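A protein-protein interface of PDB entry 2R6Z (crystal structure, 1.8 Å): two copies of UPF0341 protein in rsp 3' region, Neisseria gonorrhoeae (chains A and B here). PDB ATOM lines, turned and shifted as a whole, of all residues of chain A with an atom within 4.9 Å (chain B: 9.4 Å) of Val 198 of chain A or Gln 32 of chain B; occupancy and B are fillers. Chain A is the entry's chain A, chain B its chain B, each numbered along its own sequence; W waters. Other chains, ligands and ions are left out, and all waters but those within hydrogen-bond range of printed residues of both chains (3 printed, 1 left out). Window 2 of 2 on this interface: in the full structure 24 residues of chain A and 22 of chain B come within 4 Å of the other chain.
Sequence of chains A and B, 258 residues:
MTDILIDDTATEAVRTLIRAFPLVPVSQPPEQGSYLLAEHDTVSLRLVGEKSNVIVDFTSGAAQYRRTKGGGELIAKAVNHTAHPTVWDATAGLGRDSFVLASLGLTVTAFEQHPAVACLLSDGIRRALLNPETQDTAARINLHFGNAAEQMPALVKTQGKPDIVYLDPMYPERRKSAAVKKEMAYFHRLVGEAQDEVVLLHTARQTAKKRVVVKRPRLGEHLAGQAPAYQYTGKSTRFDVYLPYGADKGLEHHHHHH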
ATOM      1  N   ALA A 194     -16.306  28.290 -12.383  1.00  0.00           N
ATOM      2  CA  ALA A 194     -16.824  27.870 -13.676  1.00  0.00           C
ATOM      3  C   ALA A 194     -16.004  26.706 -14.230  1.00  0.00           C
ATOM      4  O   ALA A 194     -16.561  25.717 -14.707  1.00  0.00           O
ATOM      5  CB  ALA A 194     -16.802  29.037 -14.653  1.00  0.00           C
ATOM      6  N   GLN A 195     -14.683  26.828 -14.152  1.00  0.00           N
ATOM      7  CA  GLN A 195     -13.781  25.798 -14.645  1.00  0.00           C
ATOM      8  C   GLN A 195     -13.849  24.558 -13.762  1.00  0.00           C
ATOM      9  O   GLN A 195     -13.806  23.440 -14.263  1.00  0.00           O
ATOM     10  CB  GLN A 195     -12.353  26.349 -14.704  1.00  0.00           C
ATOM     11  CG  GLN A 195     -11.293  25.404 -15.249  1.00  0.00           C
ATOM     12  CD  GLN A 195     -11.649  24.829 -16.614  1.00  0.00           C
ATOM     13  OE1 GLN A 195     -12.432  25.410 -17.367  1.00  0.00           O
ATOM     14  NE2 GLN A 195     -11.063  23.687 -16.936  1.00  0.00           N
ATOM     15  N   ASP A 196     -13.960  24.750 -12.448  1.00  0.00           N
ATOM     16  CA  ASP A 196     -14.057  23.612 -11.532  1.00  0.00           C
ATOM     17  C   ASP A 196     -15.287  22.776 -11.873  1.00  0.00           C
ATOM     18  O   ASP A 196     -15.273  21.558 -11.730  1.00  0.00           O
ATOM     19  CB  ASP A 196     -14.168  24.077 -10.076  1.00  0.00           C
ATOM     20  CG  ASP A 196     -12.896  24.731  -9.565  1.00  0.00           C
ATOM     21  OD1 ASP A 196     -11.794  24.234  -9.872  1.00  0.00           O
ATOM     22  OD2 ASP A 196     -13.006  25.733  -8.834  1.00  0.00           O
ATOM     23  N   GLU A 197     -16.355  23.442 -12.305  1.00  0.00           N
ATOM     24  CA  GLU A 197     -17.595  22.755 -12.668  1.00  0.00           C
ATOM     25  C   GLU A 197     -17.358  21.872 -13.884  1.00  0.00           C
ATOM     26  O   GLU A 197     -17.806  20.723 -13.935  1.00  0.00           O
ATOM     27  CB  GLU A 197     -18.702  23.764 -12.992  1.00  0.00           C
ATOM     28  CG  GLU A 197     -19.345  24.428 -11.781  1.00  0.00           C
ATOM     29  CD  GLU A 197     -20.403  25.446 -12.183  1.00  0.00           C
ATOM     30  OE1 GLU A 197     -21.113  25.200 -13.179  1.00  0.00           O
ATOM     31  OE2 GLU A 197     -20.537  26.480 -11.501  1.00  0.00           O
ATOM     32  N   VAL A 198     -16.655  22.421 -14.868  1.00  0.00           N
ATOM     33  CA  VAL A 198     -16.351  21.682 -16.083  1.00  0.00           C
ATOM     34  C   VAL A 198     -15.555  20.433 -15.734  1.00  0.00           C
ATOM     35  O   VAL A 198     -15.861  19.344 -16.212  1.00  0.00           O
ATOM     36  CB  VAL A 198     -15.532  22.541 -17.067  1.00  0.00           C
ATOM     37  CG1 VAL A 198     -15.087  21.693 -18.249  1.00  0.00           C
ATOM     38  CG2 VAL A 198     -16.361  23.722 -17.541  1.00  0.00           C
ATOM     39  N   VAL A 199     -14.542  20.593 -14.888  1.00  0.00           N
ATOM     40  CA  VAL A 199     -13.702  19.467 -14.489  1.00  0.00           C
ATOM     41  C   VAL A 199     -14.475  18.406 -13.707  1.00  0.00           C
ATOM     42  O   VAL A 199     -14.285  17.208 -13.923  1.00  0.00           O
ATOM     43  CB  VAL A 199     -12.506  19.927 -13.620  1.00  0.00           C
ATOM     44  CG1 VAL A 199     -11.665  18.727 -13.221  1.00  0.00           C
ATOM     45  CG2 VAL A 199     -11.664  20.935 -14.385  1.00  0.00           C
ATOM     46  N   LEU A 200     -15.340  18.845 -12.797  1.00  0.00           N
ATOM     47  CA  LEU A 200     -16.127  17.918 -11.986  1.00  0.00           C
ATOM     48  C   LEU A 200     -17.040  17.047 -12.847  1.00  0.00           C
ATOM     49  O   LEU A 200     -17.040  15.822 -12.722  1.00  0.00           O
ATOM     50  CB  LEU A 200     -16.971  18.693 -10.969  1.00  0.00           C
ATOM     51  CG  LEU A 200     -17.847  17.848 -10.039  1.00  0.00           C
ATOM     52  CD1 LEU A 200     -16.995  16.812  -9.313  1.00  0.00           C
ATOM     53  CD2 LEU A 200     -18.552  18.749  -9.044  1.00  0.00           C
ATOM     54  N   LEU A 201     -17.810  17.687 -13.722  1.00  0.00           N
ATOM     55  CA  LEU A 201     -18.731  16.975 -14.600  1.00  0.00           C
ATOM     56  C   LEU A 201     -18.002  16.037 -15.558  1.00  0.00           C
ATOM     57  O   LEU A 201     -18.435  14.903 -15.784  1.00  0.00           O
ATOM     58  CB  LEU A 201     -19.572  17.971 -15.397  1.00  0.00           C
ATOM     59  CG  LEU A 201     -20.631  17.357 -16.315  1.00  0.00           C
ATOM     60  CD1 LEU A 201     -21.515  16.417 -15.505  1.00  0.00           C
ATOM     61  CD2 LEU A 201     -21.456  18.464 -16.963  1.00  0.00           C
ATOM     62  N   HIS A 202     -16.897  16.512 -16.121  1.00  0.00           N
ATOM     63  CA  HIS A 202     -16.112  15.704 -17.042  1.00  0.00           C
ATOM     64  C   HIS A 202     -15.637  14.420 -16.356  1.00  0.00           C
ATOM     65  O   HIS A 202     -15.829  13.319 -16.875  1.00  0.00           O
ATOM     66  CB  HIS A 202     -14.906  16.508 -17.552  1.00  0.00           C
ATOM     67  CG  HIS A 202     -13.938  15.696 -18.366  1.00  0.00           C
ATOM     68  ND1 HIS A 202     -14.216  15.266 -19.641  1.00  0.00           N
ATOM     69  CD2 HIS A 202     -12.720  15.201 -18.049  1.00  0.00           C
ATOM     70  CE1 HIS A 202     -13.207  14.528 -20.081  1.00  0.00           C
ATOM     71  NE2 HIS A 202     -12.290  14.472 -19.139  1.00  0.00           N
ATOM     72  N   ARG A 205     -18.458  12.001 -15.606  1.00  0.00           N
ATOM     73  CA  ARG A 205     -18.906  11.300 -16.800  1.00  0.00           C
ATOM     74  C   ARG A 205     -17.926  10.220 -17.264  1.00  0.00           C
ATOM     75  O   ARG A 205     -18.299   9.332 -18.027  1.00  0.00           O
ATOM     76  CB  ARG A 205     -19.209  12.301 -17.918  1.00  0.00           C
ATOM     77  CG  ARG A 205     -20.412  13.185 -17.600  1.00  0.00           C
ATOM     78  CD  ARG A 205     -20.739  14.138 -18.739  1.00  0.00           C
ATOM     79  NE  ARG A 205     -21.301  13.429 -19.885  1.00  0.00           N
ATOM     80  CZ  ARG A 205     -21.344  13.918 -21.119  1.00  0.00           C
ATOM     81  NH1 ARG A 205     -20.851  15.127 -21.375  1.00  0.00           N
ATOM     82  NH2 ARG A 205     -21.881  13.198 -22.095  1.00  0.00           N
ATOM     83  N   ALA A 224     -21.911  23.501 -15.627  1.00  0.00           N
ATOM     84  CA  ALA A 224     -20.898  23.624 -16.672  1.00  0.00           C
ATOM     85  C   ALA A 224     -21.517  24.051 -18.004  1.00  0.00           C
ATOM     86  O   ALA A 224     -20.912  23.882 -19.063  1.00  0.00           O
ATOM     87  CB  ALA A 224     -20.160  22.298 -16.837  1.00  0.00           C
ATOM     88  N   GLN A 226     -23.724  22.707 -19.672  1.00  0.00           N
ATOM     89  CA  GLN A 226     -23.955  21.568 -20.554  1.00  0.00           C
ATOM     90  C   GLN A 226     -25.351  20.982 -20.366  1.00  0.00           C
ATOM     91  O   GLN A 226     -25.850  20.885 -19.243  1.00  0.00           O
ATOM     92  CB  GLN A 226     -22.890  20.496 -20.308  1.00  0.00           C
ATOM     93  CG  GLN A 226     -21.475  20.987 -20.584  1.00  0.00           C
ATOM     94  CD  GLN A 226     -21.251  21.333 -22.047  1.00  0.00           C
ATOM     95  OE1 GLN A 226     -20.460  22.218 -22.375  1.00  0.00           O
ATOM     96  NE2 GLN A 226     -21.937  20.623 -22.934  1.00  0.00           N
ATOM     97  N   TYR A 245     -19.545   8.983 -20.986  1.00  0.00           N
ATOM     98  CA  TYR A 245     -19.059   9.255 -22.339  1.00  0.00           C
ATOM     99  C   TYR A 245     -19.171   8.012 -23.223  1.00  0.00           C
ATOM    100  O   TYR A 245     -18.828   6.909 -22.804  1.00  0.00           O
ATOM    101  CB  TYR A 245     -17.603   9.731 -22.304  1.00  0.00           C
ATOM    102  CG  TYR A 245     -17.432  11.168 -21.854  1.00  0.00           C
ATOM    103  CD1 TYR A 245     -18.051  12.211 -22.547  1.00  0.00           C
ATOM    104  CD2 TYR A 245     -16.619  11.489 -20.768  1.00  0.00           C
ATOM    105  CE1 TYR A 245     -17.859  13.541 -22.175  1.00  0.00           C
ATOM    106  CE2 TYR A 245     -16.420  12.815 -20.385  1.00  0.00           C
ATOM    107  CZ  TYR A 245     -17.040  13.835 -21.091  1.00  0.00           C
ATOM    108  OH  TYR A 245     -16.837  15.145 -20.723  1.00  0.00           O
ATOM    109  N   ASP B   3      -4.744  21.707 -18.103  1.00  0.00           N
ATOM    110  CA  ASP B   3      -4.184  21.200 -19.353  1.00  0.00           C
ATOM    111  C   ASP B   3      -3.354  22.282 -20.035  1.00  0.00           C
ATOM    112  O   ASP B   3      -3.662  23.476 -19.928  1.00  0.00           O
ATOM    113  CB  ASP B   3      -5.279  20.784 -20.347  1.00  0.00           C
ATOM    114  CG  ASP B   3      -6.055  19.548 -19.919  1.00  0.00           C
ATOM    115  OD1 ASP B   3      -5.541  18.731 -19.132  1.00  0.00           O
ATOM    116  OD2 ASP B   3      -7.194  19.395 -20.411  1.00  0.00           O
ATOM    117  N   GLN B  28      -4.154  17.944 -27.826  1.00  0.00           N
ATOM    118  CA  GLN B  28      -5.190  18.779 -28.416  1.00  0.00           C
ATOM    119  C   GLN B  28      -5.995  19.476 -27.327  1.00  0.00           C
ATOM    120  O   GLN B  28      -6.020  19.034 -26.179  1.00  0.00           O
ATOM    121  CB  GLN B  28      -6.130  17.942 -29.293  1.00  0.00           C
ATOM    122  CG  GLN B  28      -6.646  16.678 -28.630  1.00  0.00           C
ATOM    123  CD  GLN B  28      -7.500  15.844 -29.566  1.00  0.00           C
ATOM    124  OE1 GLN B  28      -8.713  16.040 -29.666  1.00  0.00           O
ATOM    125  NE2 GLN B  28      -6.865  14.916 -30.274  1.00  0.00           N
ATOM    126  N   PRO B  29      -6.654  20.589 -27.675  1.00  0.00           N
ATOM    127  CA  PRO B  29      -7.461  21.340 -26.716  1.00  0.00           C
ATOM    128  C   PRO B  29      -8.582  20.467 -26.160  1.00  0.00           C
ATOM    129  O   PRO B  29      -9.043  19.542 -26.820  1.00  0.00           O
ATOM    130  CB  PRO B  29      -7.999  22.494 -27.555  1.00  0.00           C
ATOM    131  CG  PRO B  29      -6.905  22.721 -28.544  1.00  0.00           C
ATOM    132  CD  PRO B  29      -6.557  21.315 -28.954  1.00  0.00           C
ATOM    133  N   PRO B  30      -9.013  20.730 -24.919  1.00  0.00           N
ATOM    134  CA  PRO B  30     -10.096  19.916 -24.366  1.00  0.00           C
ATOM    135  C   PRO B  30     -11.372  20.254 -25.128  1.00  0.00           C
ATOM    136  O   PRO B  30     -11.374  21.170 -25.952  1.00  0.00           O
ATOM    137  CB  PRO B  30     -10.147  20.352 -22.898  1.00  0.00           C
ATOM    138  CG  PRO B  30      -9.638  21.772 -22.940  1.00  0.00           C
ATOM    139  CD  PRO B  30      -8.484  21.665 -23.909  1.00  0.00           C
ATOM    140  N   GLU B  31     -12.442  19.511 -24.867  1.00  0.00           N
ATOM    141  CA  GLU B  31     -13.722  19.745 -25.532  1.00  0.00           C
ATOM    142  C   GLU B  31     -14.471  20.893 -24.876  1.00  0.00           C
ATOM    143  O   GLU B  31     -15.333  21.525 -25.493  1.00  0.00           O
ATOM    144  CB  GLU B  31     -14.599  18.488 -25.471  1.00  0.00           C
ATOM    145  CG  GLU B  31     -14.125  17.338 -26.341  1.00  0.00           C
ATOM    146  CD  GLU B  31     -14.139  17.682 -27.819  1.00  0.00           C
ATOM    147  OE1 GLU B  31     -15.218  18.025 -28.350  1.00  0.00           O
ATOM    148  OE2 GLU B  31     -13.067  17.611 -28.450  1.00  0.00           O
ATOM    149  N   GLN B  32     -14.137  21.162 -23.617  1.00  0.00           N
ATOM    150  CA  GLN B  32     -14.805  22.214 -22.869  1.00  0.00           C
ATOM    151  C   GLN B  32     -13.843  22.892 -21.906  1.00  0.00           C
ATOM    152  O   GLN B  32     -12.817  22.328 -21.528  1.00  0.00           O
ATOM    153  CB  GLN B  32     -15.948  21.622 -22.044  1.00  0.00           C
ATOM    154  CG  GLN B  32     -16.893  20.707 -22.788  1.00  0.00           C
ATOM    155  CD  GLN B  32     -17.664  19.809 -21.835  1.00  0.00           C
ATOM    156  OE1 GLN B  32     -18.274  20.283 -20.869  1.00  0.00           O
ATOM    157  NE2 GLN B  32     -17.645  18.508 -22.101  1.00  0.00           N
ATOM    158  N   GLY B  33     -14.193  24.107 -21.511  1.00  0.00           N
ATOM    159  CA  GLY B  33     -13.384  24.832 -20.553  1.00  0.00           C
ATOM    160  C   GLY B  33     -12.100  25.468 -21.032  1.00  0.00           C
ATOM    161  O   GLY B  33     -11.833  25.591 -22.228  1.00  0.00           O
ATOM    162  N   SER B  34     -11.293  25.870 -20.059  1.00  0.00           N
ATOM    163  CA  SER B  34     -10.032  26.529 -20.327  1.00  0.00           C
ATOM    164  C   SER B  34      -8.844  25.588 -20.360  1.00  0.00           C
ATOM    165  O   SER B  34      -8.931  24.415 -19.980  1.00  0.00           O
ATOM    166  CB  SER B  34      -9.781  27.598 -19.263  1.00  0.00           C
ATOM    167  OG  SER B  34      -9.657  26.992 -17.986  1.00  0.00           O
ATOM    168  N   TYR B  35      -7.722  26.134 -20.811  1.00  0.00           N
ATOM    169  CA  TYR B  35      -6.474  25.404 -20.901  1.00  0.00           C
ATOM    170  C   TYR B  35      -5.375  26.390 -21.260  1.00  0.00           C
ATOM    171  O   TYR B  35      -5.643  27.485 -21.756  1.00  0.00           O
ATOM    172  CB  TYR B  35      -6.556  24.318 -21.977  1.00  0.00           C
ATOM    173  CG  TYR B  35      -6.732  24.839 -23.394  1.00  0.00           C
ATOM    174  CD1 TYR B  35      -7.974  25.270 -23.855  1.00  0.00           C
ATOM    175  CD2 TYR B  35      -5.652  24.871 -24.277  1.00  0.00           C
ATOM    176  CE1 TYR B  35      -8.141  25.714 -25.170  1.00  0.00           C
ATOM    177  CE2 TYR B  35      -5.800  25.312 -25.593  1.00  0.00           C
ATOM    178  CZ  TYR B  35      -7.044  25.730 -26.031  1.00  0.00           C
ATOM    179  OH  TYR B  35      -7.200  26.144 -27.331  1.00  0.00           O
ATOM    180  N   ARG B  46      -6.491  30.044 -22.526  1.00  0.00           N
ATOM    181  CA  ARG B  46      -7.570  30.041 -23.505  1.00  0.00           C
ATOM    182  C   ARG B  46      -8.886  29.445 -23.014  1.00  0.00           C
ATOM    183  O   ARG B  46      -8.931  28.708 -22.027  1.00  0.00           O
ATOM    184  CB  ARG B  46      -7.142  29.227 -24.730  1.00  0.00           C
ATOM    185  CG  ARG B  46      -5.762  29.534 -25.275  1.00  0.00           C
ATOM    186  CD  ARG B  46      -5.804  30.692 -26.239  1.00  0.00           C
ATOM    187  NE  ARG B  46      -6.914  30.590 -27.188  1.00  0.00           N
ATOM    188  CZ  ARG B  46      -7.046  31.374 -28.251  1.00  0.00           C
ATOM    189  NH1 ARG B  46      -6.131  32.299 -28.495  1.00  0.00           N
ATOM    190  NH2 ARG B  46      -8.095  31.252 -29.052  1.00  0.00           N
ATOM    191  N   LEU B  47      -9.959  29.758 -23.733  1.00  0.00           N
ATOM    192  CA  LEU B  47     -11.275  29.205 -23.424  1.00  0.00           C
ATOM    193  C   LEU B  47     -11.752  28.559 -24.717  1.00  0.00           C
ATOM    194  O   LEU B  47     -11.824  29.221 -25.749  1.00  0.00           O
ATOM    195  CB  LEU B  47     -12.260  30.298 -22.998  1.00  0.00           C
ATOM    196  CG  LEU B  47     -13.711  29.856 -22.770  1.00  0.00           C
ATOM    197  CD1 LEU B  47     -13.756  28.668 -21.817  1.00  0.00           C
ATOM    198  CD2 LEU B  47     -14.516  31.017 -22.217  1.00  0.00           C
ATOM    199  N   VAL B  48     -12.051  27.264 -24.667  1.00  0.00           N
ATOM    200  CA  VAL B  48     -12.519  26.556 -25.858  1.00  0.00           C
ATOM    201  C   VAL B  48     -13.680  27.318 -26.488  1.00  0.00           C
ATOM    202  O   VAL B  48     -14.602  27.734 -25.793  1.00  0.00           O
ATOM    203  CB  VAL B  48     -12.980  25.121 -25.511  1.00  0.00           C
ATOM    204  CG1 VAL B  48     -13.592  24.446 -26.741  1.00  0.00           C
ATOM    205  CG2 VAL B  48     -11.791  24.308 -25.012  1.00  0.00           C
ATOM    206  N   GLY B  49     -13.624  27.512 -27.803  1.00  0.00           N
ATOM    207  CA  GLY B  49     -14.689  28.222 -28.492  1.00  0.00           C
ATOM    208  C   GLY B  49     -14.592  29.741 -28.479  1.00  0.00           C
ATOM    209  O   GLY B  49     -15.409  30.416 -29.110  1.00  0.00           O
HETATM  210  O   HOH W   1     -17.803  19.144 -18.437  1.00  0.00           O
HETATM  211  O   HOH W   2     -10.876  22.661 -19.668  1.00  0.00           O
HETATM  212  O   HOH W   3     -18.814  16.834 -19.548  1.00  0.00           O
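N of Ser 34 of chain B sits at hydrogen-bond distance from OE1 of Gln 195 of chain A (3.0 Å).
The side-chain amide oxygen of Gln 226 of chain A sits close to the side-chain amide oxygen of Gln 32 of chain B, at 3.3 Å.
A ring nitrogen (ND1) of His 202 of chain A is in hydrogen-bond range of the side-chain hydroxyl (OH) of Tyr 245 of chain A (2.8 Å).
O of Gly 33 of chain B is in hydrogen-bond range of N of Val 48 of chain B (3.0 Å).
The backbone carbonyl oxygen of Arg 205 of chain A lies within hydrogen-bond range of the backbone NH of Tyr 245 of chain A, 3.2 Å away.
Among the printed residues, pairs that only touch across the chains: Gln 195 of chain A with Gly 33 of chain B, Val 198 of chain A with Gln 32 of chain B and Tyr 245 of chain A with Gln 32 of chain B.
Printed residues of chain B within 4 Å of Val 198 of chain A: Gln 32 (3.9 Å).
Of the printed residues of chain A, Ser 34 of chain B touches Gln 195.
Of the printed residues of chain B, Tyr 245 of chain A touches Gln 32 (3.7 Å).
The nearest residue of chain B that does not touch Val 198 of chain A is Gly 33 of chain B (4.2 Å).
Among the printed residues, 5 pairs touch across the chains.
No position is printed for both chains.
Of the 5 pairs that touch across the chains among the printed residues, none has its exchanged pair printed and touching as well.
Water W2 lies within hydrogen-bond range of O of Ser 34 of chain B (2.6 Å), O of Gln 32 of chain B (2.7 Å) and NE2 of Gln 195 of chain A (2.9 Å).
Water W1 bridges the side-chain amide oxygen of Gln 32 of chain B and the backbone carbonyl oxygen of Val 198 of chain A.
Water W3 lies within hydrogen-bond range of the side-chain hydroxyl (OH) of Tyr 245 of chain A, the guanidinium group (NH1) of Arg 205 of chain A and the side-chain amide nitrogen (NE2) of Gln 32 of chain B.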
